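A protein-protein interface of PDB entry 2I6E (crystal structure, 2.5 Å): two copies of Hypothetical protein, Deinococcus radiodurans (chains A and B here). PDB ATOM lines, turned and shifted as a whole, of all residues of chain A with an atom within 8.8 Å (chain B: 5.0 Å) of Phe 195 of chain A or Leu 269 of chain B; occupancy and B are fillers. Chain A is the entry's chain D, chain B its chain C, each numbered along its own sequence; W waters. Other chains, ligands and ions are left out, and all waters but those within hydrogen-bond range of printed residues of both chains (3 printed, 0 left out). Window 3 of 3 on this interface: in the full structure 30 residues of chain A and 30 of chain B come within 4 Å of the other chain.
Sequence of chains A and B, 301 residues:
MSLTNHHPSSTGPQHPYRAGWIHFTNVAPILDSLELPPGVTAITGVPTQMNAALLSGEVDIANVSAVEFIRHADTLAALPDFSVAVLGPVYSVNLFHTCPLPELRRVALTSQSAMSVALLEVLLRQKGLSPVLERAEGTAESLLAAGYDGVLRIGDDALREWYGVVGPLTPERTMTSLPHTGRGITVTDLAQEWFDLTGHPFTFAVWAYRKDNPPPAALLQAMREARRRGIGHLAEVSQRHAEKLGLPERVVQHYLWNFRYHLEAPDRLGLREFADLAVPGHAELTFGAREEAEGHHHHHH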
ATOM      1  N   VAL A  86      21.993   9.431  -3.604  1.00  0.00           N
ATOM      2  CA  VAL A  86      22.835   8.641  -2.725  1.00  0.00           C
ATOM      3  C   VAL A  86      22.248   7.251  -2.501  1.00  0.00           C
ATOM      4  O   VAL A  86      21.091   6.979  -2.835  1.00  0.00           O
ATOM      5  CB  VAL A  86      22.967   9.283  -1.335  1.00  0.00           C
ATOM      6  CG1 VAL A  86      23.597  10.644  -1.447  1.00  0.00           C
ATOM      7  CG2 VAL A  86      21.606   9.374  -0.687  1.00  0.00           C
ATOM      8  N   LEU A  87      23.076   6.383  -1.932  1.00  0.00           N
ATOM      9  CA  LEU A  87      22.692   5.031  -1.577  1.00  0.00           C
ATOM     10  C   LEU A  87      23.003   4.986  -0.091  1.00  0.00           C
ATOM     11  O   LEU A  87      24.163   5.036   0.298  1.00  0.00           O
ATOM     12  CB  LEU A  87      23.550   4.008  -2.308  1.00  0.00           C
ATOM     13  CG  LEU A  87      23.187   2.565  -1.949  1.00  0.00           C
ATOM     14  CD1 LEU A  87      21.747   2.278  -2.361  1.00  0.00           C
ATOM     15  CD2 LEU A  87      24.146   1.614  -2.649  1.00  0.00           C
ATOM     16  N   GLY A  88      21.972   4.903   0.740  1.00  0.00           N
ATOM     17  CA  GLY A  88      22.192   4.894   2.171  1.00  0.00           C
ATOM     18  C   GLY A  88      21.981   6.306   2.696  1.00  0.00           C
ATOM     19  O   GLY A  88      21.167   7.051   2.145  1.00  0.00           O
ATOM     20  N   PRO A  89      22.716   6.722   3.736  1.00  0.00           N
ATOM     21  CA  PRO A  89      22.553   8.074   4.290  1.00  0.00           C
ATOM     22  C   PRO A  89      22.932   9.207   3.336  1.00  0.00           C
ATOM     23  O   PRO A  89      23.714   9.025   2.410  1.00  0.00           O
ATOM     24  CB  PRO A  89      23.455   8.050   5.523  1.00  0.00           C
ATOM     25  CG  PRO A  89      24.588   7.176   5.060  1.00  0.00           C
ATOM     26  CD  PRO A  89      23.847   6.026   4.377  1.00  0.00           C
ATOM     27  N   LEU A 119       9.121  13.271   1.378  1.00  0.00           N
ATOM     28  CA  LEU A 119       9.815  12.051   1.780  1.00  0.00           C
ATOM     29  C   LEU A 119       9.466  11.656   3.210  1.00  0.00           C
ATOM     30  O   LEU A 119       9.259  10.475   3.500  1.00  0.00           O
ATOM     31  CB  LEU A 119      11.337  12.216   1.635  1.00  0.00           C
ATOM     32  CG  LEU A 119      12.227  11.015   1.973  1.00  0.00           C
ATOM     33  CD1 LEU A 119      11.726   9.733   1.300  1.00  0.00           C
ATOM     34  CD2 LEU A 119      13.633  11.338   1.517  1.00  0.00           C
ATOM     35  N   LEU A 123       7.480   8.162   4.299  1.00  0.00           N
ATOM     36  CA  LEU A 123       8.061   7.271   5.295  1.00  0.00           C
ATOM     37  C   LEU A 123       7.174   7.103   6.526  1.00  0.00           C
ATOM     38  O   LEU A 123       6.916   5.974   6.956  1.00  0.00           O
ATOM     39  CB  LEU A 123       9.451   7.767   5.703  1.00  0.00           C
ATOM     40  CG  LEU A 123      10.503   7.666   4.588  1.00  0.00           C
ATOM     41  CD1 LEU A 123      11.773   8.418   4.972  1.00  0.00           C
ATOM     42  CD2 LEU A 123      10.803   6.205   4.313  1.00  0.00           C
ATOM     43  N   ASP A 189      18.296   9.669   9.416  1.00  0.00           N
ATOM     44  CA  ASP A 189      18.599   9.994   8.023  1.00  0.00           C
ATOM     45  C   ASP A 189      17.517   9.430   7.107  1.00  0.00           C
ATOM     46  O   ASP A 189      17.366   8.211   6.987  1.00  0.00           O
ATOM     47  CB  ASP A 189      19.961   9.391   7.676  1.00  0.00           C
ATOM     48  CG  ASP A 189      20.508   9.904   6.380  1.00  0.00           C
ATOM     49  OD1 ASP A 189      21.593  10.527   6.413  1.00  0.00           O
ATOM     50  OD2 ASP A 189      19.856   9.680   5.334  1.00  0.00           O
ATOM     51  N   LEU A 190      16.766  10.307   6.455  1.00  0.00           N
ATOM     52  CA  LEU A 190      15.688   9.842   5.590  1.00  0.00           C
ATOM     53  C   LEU A 190      16.162   9.039   4.380  1.00  0.00           C
ATOM     54  O   LEU A 190      15.447   8.162   3.903  1.00  0.00           O
ATOM     55  CB  LEU A 190      14.815  11.019   5.131  1.00  0.00           C
ATOM     56  CG  LEU A 190      14.193  11.949   6.182  1.00  0.00           C
ATOM     57  CD1 LEU A 190      13.051  12.752   5.526  1.00  0.00           C
ATOM     58  CD2 LEU A 190      13.652  11.142   7.367  1.00  0.00           C
ATOM     59  N   ALA A 191      17.353   9.324   3.868  1.00  0.00           N
ATOM     60  CA  ALA A 191      17.832   8.560   2.719  1.00  0.00           C
ATOM     61  C   ALA A 191      18.084   7.139   3.211  1.00  0.00           C
ATOM     62  O   ALA A 191      17.782   6.160   2.529  1.00  0.00           O
ATOM     63  CB  ALA A 191      19.111   9.169   2.170  1.00  0.00           C
ATOM     64  N   GLN A 192      18.630   7.036   4.416  1.00  0.00           N
ATOM     65  CA  GLN A 192      18.906   5.741   5.013  1.00  0.00           C
ATOM     66  C   GLN A 192      17.595   4.989   5.227  1.00  0.00           C
ATOM     67  O   GLN A 192      17.515   3.783   4.979  1.00  0.00           O
ATOM     68  CB  GLN A 192      19.635   5.919   6.348  1.00  0.00           C
ATOM     69  CG  GLN A 192      19.813   4.631   7.119  1.00  0.00           C
ATOM     70  CD  GLN A 192      20.516   3.573   6.303  1.00  0.00           C
ATOM     71  OE1 GLN A 192      20.424   2.379   6.601  1.00  0.00           O
ATOM     72  NE2 GLN A 192      21.238   4.003   5.268  1.00  0.00           N
ATOM     73  N   GLU A 193      16.574   5.707   5.691  1.00  0.00           N
ATOM     74  CA  GLU A 193      15.273   5.107   5.924  1.00  0.00           C
ATOM     75  C   GLU A 193      14.756   4.587   4.601  1.00  0.00           C
ATOM     76  O   GLU A 193      14.120   3.531   4.536  1.00  0.00           O
ATOM     77  CB  GLU A 193      14.304   6.135   6.527  1.00  0.00           C
ATOM     78  CG  GLU A 193      14.561   6.416   8.021  1.00  0.00           C
ATOM     79  CD  GLU A 193      14.476   5.152   8.879  1.00  0.00           C
ATOM     80  OE1 GLU A 193      15.151   5.076   9.921  1.00  0.00           O
ATOM     81  OE2 GLU A 193      13.732   4.221   8.513  1.00  0.00           O
ATOM     82  N   TRP A 194      15.054   5.323   3.536  1.00  0.00           N
ATOM     83  CA  TRP A 194      14.627   4.915   2.206  1.00  0.00           C
ATOM     84  C   TRP A 194      15.337   3.620   1.824  1.00  0.00           C
ATOM     85  O   TRP A 194      14.712   2.717   1.261  1.00  0.00           O
ATOM     86  CB  TRP A 194      14.938   6.007   1.177  1.00  0.00           C
ATOM     87  CG  TRP A 194      14.528   5.671  -0.234  1.00  0.00           C
ATOM     88  CD1 TRP A 194      15.351   5.380  -1.282  1.00  0.00           C
ATOM     89  CD2 TRP A 194      13.194   5.628  -0.752  1.00  0.00           C
ATOM     90  NE1 TRP A 194      14.617   5.167  -2.421  1.00  0.00           N
ATOM     91  CE2 TRP A 194      13.289   5.311  -2.122  1.00  0.00           C
ATOM     92  CE3 TRP A 194      11.928   5.830  -0.188  1.00  0.00           C
ATOM     93  CZ2 TRP A 194      12.167   5.191  -2.941  1.00  0.00           C
ATOM     94  CZ3 TRP A 194      10.816   5.714  -0.994  1.00  0.00           C
ATOM     95  CH2 TRP A 194      10.940   5.395  -2.363  1.00  0.00           C
ATOM     96  N   PHE A 195      16.634   3.518   2.122  1.00  0.00           N
ATOM     97  CA  PHE A 195      17.352   2.289   1.782  1.00  0.00           C
ATOM     98  C   PHE A 195      16.782   1.100   2.558  1.00  0.00           C
ATOM     99  O   PHE A 195      16.540   0.036   1.986  1.00  0.00           O
ATOM    100  CB  PHE A 195      18.854   2.386   2.066  1.00  0.00           C
ATOM    101  CG  PHE A 195      19.562   1.080   1.876  1.00  0.00           C
ATOM    102  CD1 PHE A 195      19.722   0.541   0.604  1.00  0.00           C
ATOM    103  CD2 PHE A 195      19.989   0.339   2.972  1.00  0.00           C
ATOM    104  CE1 PHE A 195      20.297  -0.725   0.428  1.00  0.00           C
ATOM    105  CE2 PHE A 195      20.565  -0.929   2.808  1.00  0.00           C
ATOM    106  CZ  PHE A 195      20.718  -1.463   1.533  1.00  0.00           C
ATOM    107  N   ASP A 196      16.583   1.282   3.862  1.00  0.00           N
ATOM    108  CA  ASP A 196      16.022   0.224   4.686  1.00  0.00           C
ATOM    109  C   ASP A 196      14.655  -0.183   4.144  1.00  0.00           C
ATOM    110  O   ASP A 196      14.229  -1.321   4.313  1.00  0.00           O
ATOM    111  CB  ASP A 196      15.878   0.668   6.150  1.00  0.00           C
ATOM    112  CG  ASP A 196      17.203   0.660   6.908  1.00  0.00           C
ATOM    113  OD1 ASP A 196      18.089  -0.162   6.583  1.00  0.00           O
ATOM    114  OD2 ASP A 196      17.358   1.467   7.851  1.00  0.00           O
ATOM    115  N   LEU A 197      13.972   0.739   3.477  1.00  0.00           N
ATOM    116  CA  LEU A 197      12.656   0.424   2.941  1.00  0.00           C
ATOM    117  C   LEU A 197      12.640  -0.157   1.528  1.00  0.00           C
ATOM    118  O   LEU A 197      11.786  -0.980   1.220  1.00  0.00           O
ATOM    119  CB  LEU A 197      11.756   1.661   2.957  1.00  0.00           C
ATOM    120  CG  LEU A 197      10.403   1.439   2.264  1.00  0.00           C
ATOM    121  CD1 LEU A 197       9.557   0.522   3.133  1.00  0.00           C
ATOM    122  CD2 LEU A 197       9.680   2.763   2.034  1.00  0.00           C
ATOM    123  N   THR A 198      13.570   0.261   0.672  1.00  0.00           N
ATOM    124  CA  THR A 198      13.572  -0.207  -0.716  1.00  0.00           C
ATOM    125  C   THR A 198      14.869  -0.871  -1.175  1.00  0.00           C
ATOM    126  O   THR A 198      14.912  -1.496  -2.238  1.00  0.00           O
ATOM    127  CB  THR A 198      13.307   0.961  -1.693  1.00  0.00           C
ATOM    128  OG1 THR A 198      14.473   1.793  -1.759  1.00  0.00           O
ATOM    129  CG2 THR A 198      12.130   1.805  -1.225  1.00  0.00           C
ATOM    130  N   GLY A 199      15.924  -0.723  -0.384  1.00  0.00           N
ATOM    131  CA  GLY A 199      17.199  -1.292  -0.762  1.00  0.00           C
ATOM    132  C   GLY A 199      17.752  -0.556  -1.969  1.00  0.00           C
ATOM    133  O   GLY A 199      18.743  -0.977  -2.553  1.00  0.00           O
ATOM    134  N   HIS A 200      17.116   0.555  -2.339  1.00  0.00           N
ATOM    135  CA  HIS A 200      17.540   1.339  -3.495  1.00  0.00           C
ATOM    136  C   HIS A 200      17.977   2.754  -3.147  1.00  0.00           C
ATOM    137  O   HIS A 200      17.670   3.268  -2.074  1.00  0.00           O
ATOM    138  CB  HIS A 200      16.412   1.412  -4.510  1.00  0.00           C
ATOM    139  CG  HIS A 200      15.976   0.076  -5.014  1.00  0.00           C
ATOM    140  ND1 HIS A 200      14.711  -0.158  -5.506  1.00  0.00           N
ATOM    141  CD2 HIS A 200      16.639  -1.103  -5.096  1.00  0.00           C
ATOM    142  CE1 HIS A 200      14.611  -1.424  -5.867  1.00  0.00           C
ATOM    143  NE2 HIS A 200      15.766  -2.019  -5.629  1.00  0.00           N
ATOM    144  N   PRO A 201      18.711   3.398  -4.061  1.00  0.00           N
ATOM    145  CA  PRO A 201      19.203   4.760  -3.878  1.00  0.00           C
ATOM    146  C   PRO A 201      18.041   5.753  -3.907  1.00  0.00           C
ATOM    147  O   PRO A 201      16.928   5.410  -4.320  1.00  0.00           O
ATOM    148  CB  PRO A 201      20.123   4.961  -5.092  1.00  0.00           C
ATOM    149  CG  PRO A 201      20.514   3.564  -5.490  1.00  0.00           C
ATOM    150  CD  PRO A 201      19.221   2.831  -5.322  1.00  0.00           C
ATOM    151  N   PHE A 202      18.298   6.978  -3.460  1.00  0.00           N
ATOM    152  CA  PHE A 202      17.270   7.992  -3.516  1.00  0.00           C
ATOM    153  C   PHE A 202      17.828   9.182  -4.280  1.00  0.00           C
ATOM    154  O   PHE A 202      18.975   9.583  -4.075  1.00  0.00           O
ATOM    155  CB  PHE A 202      16.816   8.420  -2.121  1.00  0.00           C
ATOM    156  CG  PHE A 202      15.581   9.268  -2.134  1.00  0.00           C
ATOM    157  CD1 PHE A 202      15.669  10.646  -2.354  1.00  0.00           C
ATOM    158  CD2 PHE A 202      14.315   8.676  -2.006  1.00  0.00           C
ATOM    159  CE1 PHE A 202      14.521  11.423  -2.448  1.00  0.00           C
ATOM    160  CE2 PHE A 202      13.155   9.441  -2.097  1.00  0.00           C
ATOM    161  CZ  PHE A 202      13.254  10.818  -2.321  1.00  0.00           C
ATOM    162  N   GLU A 273      10.491   4.837  -8.088  1.00  0.00           N
ATOM    163  CA  GLU A 273       9.897   4.191  -6.930  1.00  0.00           C
ATOM    164  C   GLU A 273       9.230   5.274  -6.091  1.00  0.00           C
ATOM    165  O   GLU A 273       8.051   5.177  -5.732  1.00  0.00           O
ATOM    166  CB  GLU A 273      10.983   3.486  -6.122  1.00  0.00           C
ATOM    167  CG  GLU A 273      10.688   2.045  -5.828  1.00  0.00           C
ATOM    168  CD  GLU A 273      11.946   1.203  -5.731  1.00  0.00           C
ATOM    169  OE1 GLU A 273      12.871   1.592  -4.981  1.00  0.00           O
ATOM    170  OE2 GLU A 273      12.003   0.150  -6.407  1.00  0.00           O
ATOM    171  N   HIS B 200      20.968  -4.461  -6.050  1.00  0.00           N
ATOM    172  CA  HIS B 200      21.910  -4.099  -4.987  1.00  0.00           C
ATOM    173  C   HIS B 200      23.359  -4.000  -5.475  1.00  0.00           C
ATOM    174  O   HIS B 200      23.685  -4.374  -6.600  1.00  0.00           O
ATOM    175  CB  HIS B 200      21.835  -5.130  -3.857  1.00  0.00           C
ATOM    176  CG  HIS B 200      20.460  -5.318  -3.295  1.00  0.00           C
ATOM    177  ND1 HIS B 200      20.030  -6.514  -2.759  1.00  0.00           N
ATOM    178  CD2 HIS B 200      19.422  -4.455  -3.164  1.00  0.00           C
ATOM    179  CE1 HIS B 200      18.789  -6.380  -2.325  1.00  0.00           C
ATOM    180  NE2 HIS B 200      18.397  -5.141  -2.557  1.00  0.00           N
ATOM    181  N   GLU B 264      29.724  -0.501   3.335  1.00  0.00           N
ATOM    182  CA  GLU B 264      28.553  -0.090   4.094  1.00  0.00           C
ATOM    183  C   GLU B 264      27.406  -1.104   3.996  1.00  0.00           C
ATOM    184  O   GLU B 264      27.494  -2.106   3.275  1.00  0.00           O
ATOM    185  CB  GLU B 264      28.087   1.277   3.599  1.00  0.00           C
ATOM    186  CG  GLU B 264      29.100   2.385   3.815  1.00  0.00           C
ATOM    187  CD  GLU B 264      28.686   3.689   3.149  1.00  0.00           C
ATOM    188  OE1 GLU B 264      29.130   3.954   2.008  1.00  0.00           O
ATOM    189  OE2 GLU B 264      27.899   4.450   3.766  1.00  0.00           O
ATOM    190  N   ALA B 265      26.322  -0.825   4.714  1.00  0.00           N
ATOM    191  CA  ALA B 265      25.156  -1.711   4.735  1.00  0.00           C
ATOM    192  C   ALA B 265      24.752  -2.242   3.352  1.00  0.00           C
ATOM    193  O   ALA B 265      24.583  -3.448   3.176  1.00  0.00           O
ATOM    194  CB  ALA B 265      23.967  -1.007   5.404  1.00  0.00           C
ATOM    195  N   PRO B 266      24.574  -1.350   2.362  1.00  0.00           N
ATOM    196  CA  PRO B 266      24.190  -1.800   1.013  1.00  0.00           C
ATOM    197  C   PRO B 266      25.218  -2.786   0.439  1.00  0.00           C
ATOM    198  O   PRO B 266      24.862  -3.810  -0.150  1.00  0.00           O
ATOM    199  CB  PRO B 266      24.135  -0.502   0.210  1.00  0.00           C
ATOM    200  CG  PRO B 266      23.775   0.522   1.247  1.00  0.00           C
ATOM    201  CD  PRO B 266      24.634   0.120   2.429  1.00  0.00           C
ATOM    202  N   ASP B 267      26.496  -2.481   0.617  1.00  0.00           N
ATOM    203  CA  ASP B 267      27.538  -3.363   0.109  1.00  0.00           C
ATOM    204  C   ASP B 267      27.494  -4.724   0.801  1.00  0.00           C
ATOM    205  O   ASP B 267      27.620  -5.757   0.142  1.00  0.00           O
ATOM    206  CB  ASP B 267      28.913  -2.711   0.290  1.00  0.00           C
ATOM    207  CG  ASP B 267      28.940  -1.299  -0.239  1.00  0.00           C
ATOM    208  OD1 ASP B 267      28.620  -1.134  -1.430  1.00  0.00           O
ATOM    209  OD2 ASP B 267      29.260  -0.359   0.526  1.00  0.00           O
ATOM    210  N   ARG B 268      27.310  -4.725   2.124  1.00  0.00           N
ATOM    211  CA  ARG B 268      27.253  -5.975   2.879  1.00  0.00           C
ATOM    212  C   ARG B 268      26.014  -6.772   2.465  1.00  0.00           C
ATOM    213  O   ARG B 268      26.024  -8.005   2.474  1.00  0.00           O
ATOM    214  CB  ARG B 268      27.233  -5.697   4.385  1.00  0.00           C
ATOM    215  CG  ARG B 268      28.241  -4.637   4.800  1.00  0.00           C
ATOM    216  CD  ARG B 268      29.197  -5.073   5.903  1.00  0.00           C
ATOM    217  NE  ARG B 268      28.821  -4.574   7.223  1.00  0.00           N
ATOM    218  CZ  ARG B 268      29.686  -4.277   8.192  1.00  0.00           C
ATOM    219  NH1 ARG B 268      30.994  -4.413   8.011  1.00  0.00           N
ATOM    220  NH2 ARG B 268      29.242  -3.855   9.364  1.00  0.00           N
ATOM    221  N   LEU B 269      24.952  -6.066   2.084  1.00  0.00           N
ATOM    222  CA  LEU B 269      23.732  -6.732   1.654  1.00  0.00           C
ATOM    223  C   LEU B 269      24.061  -7.534   0.397  1.00  0.00           C
ATOM    224  O   LEU B 269      23.772  -8.727   0.308  1.00  0.00           O
ATOM    225  CB  LEU B 269      22.632  -5.707   1.351  1.00  0.00           C
ATOM    226  CG  LEU B 269      21.273  -6.270   0.889  1.00  0.00           C
ATOM    227  CD1 LEU B 269      20.718  -7.212   1.949  1.00  0.00           C
ATOM    228  CD2 LEU B 269      20.279  -5.129   0.631  1.00  0.00           C
ATOM    229  N   GLY B 270      24.680  -6.871  -0.573  1.00  0.00           N
ATOM    230  CA  GLY B 270      25.039  -7.545  -1.800  1.00  0.00           C
ATOM    231  C   GLY B 270      25.980  -8.700  -1.524  1.00  0.00           C
ATOM    232  O   GLY B 270      25.797  -9.796  -2.057  1.00  0.00           O
ATOM    233  N   LEU B 271      26.980  -8.455  -0.680  1.00  0.00           N
ATOM    234  CA  LEU B 271      27.960  -9.474  -0.342  1.00  0.00           C
ATOM    235  C   LEU B 271      27.289 -10.739   0.177  1.00  0.00           C
ATOM    236  O   LEU B 271      27.570 -11.830  -0.302  1.00  0.00           O
ATOM    237  CB  LEU B 271      28.946  -8.940   0.698  1.00  0.00           C
ATOM    238  CG  LEU B 271      30.082  -9.887   1.116  1.00  0.00           C
ATOM    239  CD1 LEU B 271      30.912 -10.307  -0.097  1.00  0.00           C
ATOM    240  CD2 LEU B 271      30.960  -9.191   2.146  1.00  0.00           C
ATOM    241  N   ARG B 272      26.396 -10.594   1.151  1.00  0.00           N
ATOM    242  CA  ARG B 272      25.707 -11.746   1.706  1.00  0.00           C
ATOM    243  C   ARG B 272      24.825 -12.436   0.674  1.00  0.00           C
ATOM    244  O   ARG B 272      24.813 -13.664   0.598  1.00  0.00           O
ATOM    245  CB  ARG B 272      24.857 -11.352   2.921  1.00  0.00           C
ATOM    246  CG  ARG B 272      25.665 -11.016   4.174  1.00  0.00           C
ATOM    247  CD  ARG B 272      24.758 -10.849   5.384  1.00  0.00           C
ATOM    248  NE  ARG B 272      23.828  -9.730   5.224  1.00  0.00           N
ATOM    249  CZ  ARG B 272      24.124  -8.465   5.511  1.00  0.00           C
ATOM    250  NH1 ARG B 272      25.331  -8.155   5.984  1.00  0.00           N
ATOM    251  NH2 ARG B 272      23.216  -7.512   5.318  1.00  0.00           N
ATOM    252  N   GLU B 273      24.087 -11.670  -0.123  1.00  0.00           N
ATOM    253  CA  GLU B 273      23.231 -12.302  -1.124  1.00  0.00           C
ATOM    254  C   GLU B 273      24.054 -13.182  -2.051  1.00  0.00           C
ATOM    255  O   GLU B 273      23.622 -14.273  -2.432  1.00  0.00           O
ATOM    256  CB  GLU B 273      22.473 -11.257  -1.939  1.00  0.00           C
ATOM    257  CG  GLU B 273      21.523 -10.448  -1.093  1.00  0.00           C
ATOM    258  CD  GLU B 273      20.717  -9.446  -1.894  1.00  0.00           C
ATOM    259  OE1 GLU B 273      21.304  -8.761  -2.762  1.00  0.00           O
ATOM    260  OE2 GLU B 273      19.497  -9.334  -1.642  1.00  0.00           O
HETATM  261  O   HOH W   1      27.389   5.030   0.193  1.00  0.00           O
HETATM  262  O   HOH W   2      15.939  -4.210  -2.182  1.00  0.00           O
HETATM  263  O   HOH W   3      25.756   3.499   1.948  1.00  0.00           O
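A ring nitrogen (ND1) of His 200 of chain B is in hydrogen-bond range of the side-chain carboxylate of Glu 273 of chain B, 2.6 Å away.
Printed residues of chain A that touch a printed residue of chain B: Leu 87, Phe 195 and Gly 199. Hydrophobic or aromatic side chains of chain A within 4 Å of the printed part of chain B: Leu 87 and Phe 195. Printed residues of chain B that touch a printed residue of chain A: His 200, Pro 266 and Leu 269. Hydrophobic or aromatic side chains of chain B within 4 Å of the printed part of chain A: His 200, Pro 266 and Leu 269. Among the printed residues, 4 pairs touch across the chains.
Water W2 lies within hydrogen-bond range of NE2 of His 200 of chain B (2.7 Å) and O of Thr 198 of chain A (2.9 Å). Water W1 bridges OE1 of Glu 264 of chain B and O of Leu 87 of chain A. Water W3 bridges O of Leu 87 of chain A (2.8 Å) and OE2 of Glu 264 of chain B (3.0 Å).
Phe 195 of chain A touches just these residues of chain B: Pro 266 (3.5 Å) and Leu 269 (3.8 Å). Leu 269 of chain B touches one residue of chain A. Of chain A, only Leu 87 (3.6 Å) and Phe 195 (3.5 Å) come within 4 Å of Pro 266 of chain B. Gly 270 of chain B touches none of the printed residues of chain A. Of the printed residues of chain B, Gly 199 of chain A touches His 200. Of the printed residues of chain B, Leu 87 of chain A touches Pro 266. The nearest residue of chain B that does not touch Phe 195 of chain A is Ala 265 of chain B (4.3 Å). The nearest printed residue of chain B that does not touch Leu 87 of chain A is Glu 264 of chain B (5.1 Å).
Pro 266 of chain B touches Leu 87 of chain A (CB to CD2, 3.6 Å). Pro 266 of chain B touches Phe 195 of chain A (CA to CZ, 3.5 Å). Leu 269 of chain B touches Phe 195 of chain A. Gly 199 of chain A touches His 200 of chain B (O to CD2, 3.6 Å).
2 positions are printed for both chains. Of the 4 pairs that touch across the chains among the printed residues, none has its exchanged pair printed and touching as well.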
